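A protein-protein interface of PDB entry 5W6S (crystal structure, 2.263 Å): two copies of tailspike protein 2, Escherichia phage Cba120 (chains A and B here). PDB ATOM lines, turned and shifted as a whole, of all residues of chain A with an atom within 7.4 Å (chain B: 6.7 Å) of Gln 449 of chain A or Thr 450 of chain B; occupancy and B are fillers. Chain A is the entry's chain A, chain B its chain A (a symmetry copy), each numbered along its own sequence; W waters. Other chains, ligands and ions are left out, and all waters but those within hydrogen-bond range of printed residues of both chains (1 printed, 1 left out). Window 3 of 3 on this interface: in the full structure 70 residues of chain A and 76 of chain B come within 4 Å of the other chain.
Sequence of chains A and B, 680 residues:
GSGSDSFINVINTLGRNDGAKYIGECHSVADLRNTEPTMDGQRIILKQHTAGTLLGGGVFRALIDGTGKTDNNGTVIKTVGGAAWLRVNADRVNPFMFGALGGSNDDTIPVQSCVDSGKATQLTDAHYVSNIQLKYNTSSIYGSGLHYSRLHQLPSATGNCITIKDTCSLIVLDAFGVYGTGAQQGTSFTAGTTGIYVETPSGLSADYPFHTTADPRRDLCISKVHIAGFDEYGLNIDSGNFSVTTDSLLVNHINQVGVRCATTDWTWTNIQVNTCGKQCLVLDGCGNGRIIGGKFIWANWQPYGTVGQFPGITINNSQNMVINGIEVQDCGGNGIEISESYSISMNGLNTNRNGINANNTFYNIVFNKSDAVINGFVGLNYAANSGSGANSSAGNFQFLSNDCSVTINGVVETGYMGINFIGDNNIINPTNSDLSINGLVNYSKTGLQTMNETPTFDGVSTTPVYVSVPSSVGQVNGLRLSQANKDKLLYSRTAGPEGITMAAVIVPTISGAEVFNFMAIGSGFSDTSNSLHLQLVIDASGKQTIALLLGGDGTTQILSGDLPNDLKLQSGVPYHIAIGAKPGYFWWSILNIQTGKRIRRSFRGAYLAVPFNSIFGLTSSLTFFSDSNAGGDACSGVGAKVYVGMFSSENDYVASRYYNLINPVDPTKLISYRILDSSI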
ATOM      1  N   THR A 446     -12.153 -35.265 -28.669  1.00  0.00           N
ATOM      2  CA  THR A 446     -12.340 -33.855 -28.365  1.00  0.00           C
ATOM      3  C   THR A 446     -11.016 -33.155 -28.095  1.00  0.00           C
ATOM      4  O   THR A 446     -10.106 -33.723 -27.485  1.00  0.00           O
ATOM      5  CB  THR A 446     -13.274 -33.659 -27.168  1.00  0.00           C
ATOM      6  OG1 THR A 446     -13.517 -32.259 -26.998  1.00  0.00           O
ATOM      7  CG2 THR A 446     -12.651 -34.211 -25.896  1.00  0.00           C
ATOM      8  N   GLY A 447     -10.924 -31.909 -28.553  1.00  0.00           N
ATOM      9  CA  GLY A 447      -9.864 -31.005 -28.162  1.00  0.00           C
ATOM     10  C   GLY A 447     -10.294 -29.939 -27.176  1.00  0.00           C
ATOM     11  O   GLY A 447      -9.543 -28.980 -26.957  1.00  0.00           O
ATOM     12  N   LEU A 448     -11.477 -30.077 -26.576  1.00  0.00           N
ATOM     13  CA  LEU A 448     -11.998 -29.053 -25.683  1.00  0.00           C
ATOM     14  C   LEU A 448     -11.127 -28.924 -24.439  1.00  0.00           C
ATOM     15  O   LEU A 448     -10.677 -29.920 -23.864  1.00  0.00           O
ATOM     16  CB  LEU A 448     -13.434 -29.391 -25.285  1.00  0.00           C
ATOM     17  CG  LEU A 448     -14.473 -29.314 -26.410  1.00  0.00           C
ATOM     18  CD1 LEU A 448     -15.799 -29.957 -25.989  1.00  0.00           C
ATOM     19  CD2 LEU A 448     -14.692 -27.867 -26.834  1.00  0.00           C
ATOM     20  N   GLN A 449     -10.890 -27.685 -24.021  1.00  0.00           N
ATOM     21  CA  GLN A 449     -10.174 -27.425 -22.782  1.00  0.00           C
ATOM     22  C   GLN A 449     -11.175 -27.368 -21.639  1.00  0.00           C
ATOM     23  O   GLN A 449     -12.215 -26.713 -21.748  1.00  0.00           O
ATOM     24  CB  GLN A 449      -9.375 -26.124 -22.863  1.00  0.00           C
ATOM     25  CG  GLN A 449      -8.273 -26.156 -23.910  1.00  0.00           C
ATOM     26  CD  GLN A 449      -7.419 -27.416 -23.819  1.00  0.00           C
ATOM     27  OE1 GLN A 449      -6.406 -27.445 -23.117  1.00  0.00           O
ATOM     28  NE2 GLN A 449      -7.831 -28.469 -24.528  1.00  0.00           N
ATOM     29  N   THR A 450     -10.861 -28.065 -20.551  1.00  0.00           N
ATOM     30  CA  THR A 450     -11.730 -28.142 -19.388  1.00  0.00           C
ATOM     31  C   THR A 450     -10.920 -27.850 -18.134  1.00  0.00           C
ATOM     32  O   THR A 450      -9.689 -27.857 -18.152  1.00  0.00           O
ATOM     33  CB  THR A 450     -12.382 -29.532 -19.256  1.00  0.00           C
ATOM     34  OG1 THR A 450     -11.401 -30.474 -18.809  1.00  0.00           O
ATOM     35  CG2 THR A 450     -12.937 -30.002 -20.594  1.00  0.00           C
ATOM     36  N   MET A 451     -11.634 -27.572 -17.045  1.00  0.00           N
ATOM     37  CA  MET A 451     -11.038 -27.671 -15.723  1.00  0.00           C
ATOM     38  C   MET A 451     -10.352 -29.019 -15.562  1.00  0.00           C
ATOM     39  O   MET A 451     -10.779 -30.028 -16.134  1.00  0.00           O
ATOM     40  CB  MET A 451     -12.096 -27.568 -14.626  1.00  0.00           C
ATOM     41  CG  MET A 451     -12.974 -26.360 -14.628  1.00  0.00           C
ATOM     42  SD  MET A 451     -14.093 -26.574 -13.233  1.00  0.00           S
ATOM     43  CE  MET A 451     -12.938 -26.523 -11.858  1.00  0.00           C
ATOM     44  N   ASN A 452      -9.311 -29.046 -14.734  1.00  0.00           N
ATOM     45  CA  ASN A 452      -8.790 -30.331 -14.268  1.00  0.00           C
ATOM     46  C   ASN A 452      -8.218 -30.111 -12.867  1.00  0.00           C
ATOM     47  O   ASN A 452      -7.026 -29.840 -12.704  1.00  0.00           O
ATOM     48  CB  ASN A 452      -7.756 -30.911 -15.217  1.00  0.00           C
ATOM     49  CG  ASN A 452      -7.586 -32.403 -15.022  1.00  0.00           C
ATOM     50  OD1 ASN A 452      -7.861 -32.932 -13.940  1.00  0.00           O
ATOM     51  ND2 ASN A 452      -7.150 -33.093 -16.066  1.00  0.00           N
ATOM     52  N   PRO A 667     -17.234 -35.035 -21.328  1.00  0.00           N
ATOM     53  CA  PRO A 667     -16.287 -33.903 -21.394  1.00  0.00           C
ATOM     54  C   PRO A 667     -16.885 -32.559 -20.991  1.00  0.00           C
ATOM     55  O   PRO A 667     -16.171 -31.739 -20.399  1.00  0.00           O
ATOM     56  CB  PRO A 667     -15.839 -33.914 -22.863  1.00  0.00           C
ATOM     57  CG  PRO A 667     -15.945 -35.354 -23.268  1.00  0.00           C
ATOM     58  CD  PRO A 667     -17.172 -35.888 -22.528  1.00  0.00           C
ATOM     59  N   TYR B 443     -18.752 -22.608 -35.400  1.00  0.00           N
ATOM     60  CA  TYR B 443     -17.495 -22.000 -34.967  1.00  0.00           C
ATOM     61  C   TYR B 443     -17.621 -20.487 -34.846  1.00  0.00           C
ATOM     62  O   TYR B 443     -17.013 -19.878 -33.959  1.00  0.00           O
ATOM     63  CB  TYR B 443     -16.361 -22.368 -35.920  1.00  0.00           C
ATOM     64  CG  TYR B 443     -15.030 -21.770 -35.507  1.00  0.00           C
ATOM     65  CD1 TYR B 443     -14.248 -22.371 -34.516  1.00  0.00           C
ATOM     66  CD2 TYR B 443     -14.558 -20.597 -36.092  1.00  0.00           C
ATOM     67  CE1 TYR B 443     -13.028 -21.823 -34.132  1.00  0.00           C
ATOM     68  CE2 TYR B 443     -13.343 -20.039 -35.710  1.00  0.00           C
ATOM     69  CZ  TYR B 443     -12.585 -20.660 -34.735  1.00  0.00           C
ATOM     70  OH  TYR B 443     -11.384 -20.114 -34.363  1.00  0.00           O
ATOM     71  N   GLY B 447     -17.350 -19.444 -27.962  1.00  0.00           N
ATOM     72  CA  GLY B 447     -16.207 -18.997 -27.197  1.00  0.00           C
ATOM     73  C   GLY B 447     -15.417 -20.118 -26.554  1.00  0.00           C
ATOM     74  O   GLY B 447     -14.571 -19.845 -25.693  1.00  0.00           O
ATOM     75  N   LEU B 448     -15.667 -21.368 -26.945  1.00  0.00           N
ATOM     76  CA  LEU B 448     -15.013 -22.505 -26.314  1.00  0.00           C
ATOM     77  C   LEU B 448     -13.512 -22.482 -26.578  1.00  0.00           C
ATOM     78  O   LEU B 448     -13.058 -22.185 -27.687  1.00  0.00           O
ATOM     79  CB  LEU B 448     -15.616 -23.808 -26.836  1.00  0.00           C
ATOM     80  CG  LEU B 448     -17.069 -24.080 -26.428  1.00  0.00           C
ATOM     81  CD1 LEU B 448     -17.669 -25.235 -27.239  1.00  0.00           C
ATOM     82  CD2 LEU B 448     -17.158 -24.373 -24.936  1.00  0.00           C
ATOM     83  N   GLN B 449     -12.736 -22.799 -25.546  1.00  0.00           N
ATOM     84  CA  GLN B 449     -11.295 -22.929 -25.692  1.00  0.00           C
ATOM     85  C   GLN B 449     -10.968 -24.364 -26.077  1.00  0.00           C
ATOM     86  O   GLN B 449     -11.486 -25.308 -25.473  1.00  0.00           O
ATOM     87  CB  GLN B 449     -10.567 -22.539 -24.405  1.00  0.00           C
ATOM     88  CG  GLN B 449     -10.754 -21.079 -24.024  1.00  0.00           C
ATOM     89  CD  GLN B 449     -10.512 -20.135 -25.198  1.00  0.00           C
ATOM     90  OE1 GLN B 449      -9.390 -19.672 -25.416  1.00  0.00           O
ATOM     91  NE2 GLN B 449     -11.568 -19.850 -25.963  1.00  0.00           N
ATOM     92  N   THR B 450     -10.119 -24.519 -27.088  1.00  0.00           N
ATOM     93  CA  THR B 450      -9.735 -25.824 -27.599  1.00  0.00           C
ATOM     94  C   THR B 450      -8.220 -25.894 -27.715  1.00  0.00           C
ATOM     95  O   THR B 450      -7.527 -24.878 -27.657  1.00  0.00           O
ATOM     96  CB  THR B 450     -10.361 -26.102 -28.980  1.00  0.00           C
ATOM     97  OG1 THR B 450      -9.688 -25.317 -29.970  1.00  0.00           O
ATOM     98  CG2 THR B 450     -11.840 -25.738 -28.990  1.00  0.00           C
ATOM     99  N   MET B 451      -7.714 -27.118 -27.860  1.00  0.00           N
ATOM    100  CA  MET B 451      -6.369 -27.307 -28.377  1.00  0.00           C
ATOM    101  C   MET B 451      -6.191 -26.517 -29.665  1.00  0.00           C
ATOM    102  O   MET B 451      -7.138 -26.326 -30.437  1.00  0.00           O
ATOM    103  CB  MET B 451      -6.099 -28.773 -28.705  1.00  0.00           C
ATOM    104  CG  MET B 451      -6.300 -29.772 -27.614  1.00  0.00           C
ATOM    105  SD  MET B 451      -5.914 -31.372 -28.344  1.00  0.00           S
ATOM    106  CE  MET B 451      -4.167 -31.168 -28.712  1.00  0.00           C
ATOM    107  N   ASN B 452      -4.955 -26.097 -29.924  1.00  0.00           N
ATOM    108  CA  ASN B 452      -4.619 -25.618 -31.264  1.00  0.00           C
ATOM    109  C   ASN B 452      -3.145 -25.943 -31.510  1.00  0.00           C
ATOM    110  O   ASN B 452      -2.263 -25.120 -31.254  1.00  0.00           O
ATOM    111  CB  ASN B 452      -4.909 -24.137 -31.435  1.00  0.00           C
ATOM    112  CG  ASN B 452      -5.038 -23.753 -32.893  1.00  0.00           C
ATOM    113  OD1 ASN B 452      -4.490 -24.425 -33.773  1.00  0.00           O
ATOM    114  ND2 ASN B 452      -5.774 -22.684 -33.164  1.00  0.00           N
ATOM    115  N   PRO B 667     -16.162 -27.680 -33.666  1.00  0.00           N
ATOM    116  CA  PRO B 667     -15.381 -27.138 -32.537  1.00  0.00           C
ATOM    117  C   PRO B 667     -15.071 -28.153 -31.442  1.00  0.00           C
ATOM    118  O   PRO B 667     -13.991 -28.074 -30.841  1.00  0.00           O
ATOM    119  CB  PRO B 667     -16.267 -25.993 -32.023  1.00  0.00           C
ATOM    120  CG  PRO B 667     -17.009 -25.529 -33.242  1.00  0.00           C
ATOM    121  CD  PRO B 667     -17.276 -26.796 -34.054  1.00  0.00           C
ATOM    122  N   THR B 668     -15.968 -29.107 -31.163  1.00  0.00           N
ATOM    123  CA  THR B 668     -15.692 -30.081 -30.110  1.00  0.00           C
ATOM    124  C   THR B 668     -14.652 -31.110 -30.529  1.00  0.00           C
ATOM    125  O   THR B 668     -14.159 -31.849 -29.668  1.00  0.00           O
ATOM    126  CB  THR B 668     -16.971 -30.812 -29.670  1.00  0.00           C
ATOM    127  OG1 THR B 668     -17.394 -31.712 -30.703  1.00  0.00           O
ATOM    128  CG2 THR B 668     -18.095 -29.823 -29.379  1.00  0.00           C
ATOM    129  N   LYS B 669     -14.314 -31.179 -31.817  1.00  0.00           N
ATOM    130  CA  LYS B 669     -13.296 -32.091 -32.318  1.00  0.00           C
ATOM    131  C   LYS B 669     -12.061 -31.363 -32.837  1.00  0.00           C
ATOM    132  O   LYS B 669     -11.154 -32.009 -33.370  1.00  0.00           O
ATOM    133  CB  LYS B 669     -13.881 -32.976 -33.432  1.00  0.00           C
ATOM    134  CG  LYS B 669     -15.047 -33.878 -33.006  1.00  0.00           C
ATOM    135  CD  LYS B 669     -15.616 -34.644 -34.200  1.00  0.00           C
ATOM    136  CE  LYS B 669     -16.748 -35.594 -33.782  1.00  0.00           C
ATOM    137  NZ  LYS B 669     -17.376 -36.294 -34.956  1.00  0.00           N
ATOM    138  N   LEU B 670     -11.999 -30.044 -32.687  1.00  0.00           N
ATOM    139  CA  LEU B 670     -10.920 -29.264 -33.278  1.00  0.00           C
ATOM    140  C   LEU B 670      -9.592 -29.548 -32.578  1.00  0.00           C
ATOM    141  O   LEU B 670      -9.489 -29.480 -31.348  1.00  0.00           O
ATOM    142  CB  LEU B 670     -11.266 -27.778 -33.208  1.00  0.00           C
ATOM    143  CG  LEU B 670     -10.391 -26.729 -33.896  1.00  0.00           C
ATOM    144  CD1 LEU B 670     -11.215 -25.463 -34.104  1.00  0.00           C
ATOM    145  CD2 LEU B 670      -9.140 -26.418 -33.083  1.00  0.00           C
ATOM    146  N   ILE B 671      -8.579 -29.883 -33.373  1.00  0.00           N
ATOM    147  CA  ILE B 671      -7.237 -30.118 -32.873  1.00  0.00           C
ATOM    148  C   ILE B 671      -6.282 -29.001 -33.269  1.00  0.00           C
ATOM    149  O   ILE B 671      -5.353 -28.691 -32.511  1.00  0.00           O
ATOM    150  CB  ILE B 671      -6.708 -31.479 -33.378  1.00  0.00           C
ATOM    151  CG1 ILE B 671      -7.621 -32.635 -32.934  1.00  0.00           C
ATOM    152  CG2 ILE B 671      -5.225 -31.660 -33.008  1.00  0.00           C
ATOM    153  CD1 ILE B 671      -7.997 -32.603 -31.455  1.00  0.00           C
ATOM    154  N   SER B 672      -6.469 -28.405 -34.441  1.00  0.00           N
ATOM    155  CA  SER B 672      -5.627 -27.320 -34.910  1.00  0.00           C
ATOM    156  C   SER B 672      -6.429 -26.494 -35.901  1.00  0.00           C
ATOM    157  O   SER B 672      -7.247 -27.035 -36.657  1.00  0.00           O
ATOM    158  CB  SER B 672      -4.344 -27.839 -35.568  1.00  0.00           C
ATOM    159  OG  SER B 672      -3.522 -26.758 -35.979  1.00  0.00           O
HETATM  160  O   HOH W   1     -13.979 -25.799 -23.948  1.00  0.00           O
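O of Gly 447 of chain A is in hydrogen-bond range of NE2 of Gln 449 of chain A, at 3.0 Å.
N of Leu 448 of chain A is in hydrogen-bond range of OG1 of Thr 446 of chain A.
The side-chain amide nitrogen (NE2) of Gln 449 of chain B sits at hydrogen-bond distance from the backbone carbonyl oxygen (O) of Gly 447 of chain B, 3.0 Å away.
Of the 8 printed residues of chain A, 4 touch a printed residue of chain B.
Printed residues of chain A that touch a printed residue of chain B: Thr 446, Gly 447, Leu 448 and Gln 449.
Hydrophobic or aromatic side chains of chain A that line the printed part of chain B: Leu 448.
Along chain B the printed residues that touch a printed residue of chain A span positions 448 to 670.
Gly 447 of chain A touches Thr 450 of chain B, but with the chains exchanged Thr 450 of chain A does not touch Gly 447 of chain B (10.4 Å).
Gly 447 of chain A touches Met 451 of chain B, but with the chains exchanged Met 451 of chain A does not touch Gly 447 of chain B (12.0 Å).
Leu 448 of chain A touches its own counterpart, Leu 448 of chain B.
Gln 449 of chain A touches Met 451 of chain B, but with the chains exchanged Met 451 of chain A does not touch Gln 449 of chain B (8.7 Å).
7 positions are printed for both chains.
Of the printed residues of chain B, Gly 447 of chain A touches Thr 450, Met 451, Thr 668 and Leu 670.
Of the printed residues of chain B, Leu 448 of chain A touches Leu 448 (3.99 Å), Gln 449 (3.8 Å) and Thr 668 (3.96 Å).
Of chain B, only Gln 449 (2.8 Å), Thr 450 (3.8 Å) and Met 451 (3.6 Å) come within 4 Å of Gln 449 of chain A.
Met 451 of chain A touches none of the printed residues of chain B.
The nearest residue of chain B that does not touch Gln 449 of chain A is Leu 448 of chain B (6.3 Å).
The nearest printed residue of chain A that does not touch Leu 448 of chain B is Gln 449 of chain A (6.3 Å).
The backbone NH (N) of Gln 449 of chain A sits at hydrogen-bond distance from the backbone carbonyl oxygen (O) of Gln 449 of chain B (2.8 Å).
The backbone NH of Met 451 of chain B sits at hydrogen-bond distance from the backbone carbonyl oxygen of Gly 447 of chain A, at 2.8 Å.
O of Thr 668 of chain B is in hydrogen-bond range of N of Gly 447 of chain A, 3.4 Å away.
O of Thr 668 of chain B sits at hydrogen-bond distance from OG1 of Thr 446 of chain A.
Water W1 bridges O of Gln 449 of chain A and O of Gln 449 of chain B.
Among the printed residues, merely in contact across the chains: Gly 447 of chain A with Thr 450 of chain B, Gly 447 of chain A with Leu 670 of chain B, Gln 449 of chain A with Met 451 of chain B, Leu 448 of chain A with Gln 449 of chain B, Gln 449 of chain A with Thr 450 of chain B, Leu 448 of chain A with Thr 668 of chain B and Leu 448 of chain A with Leu 448 of chain B.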
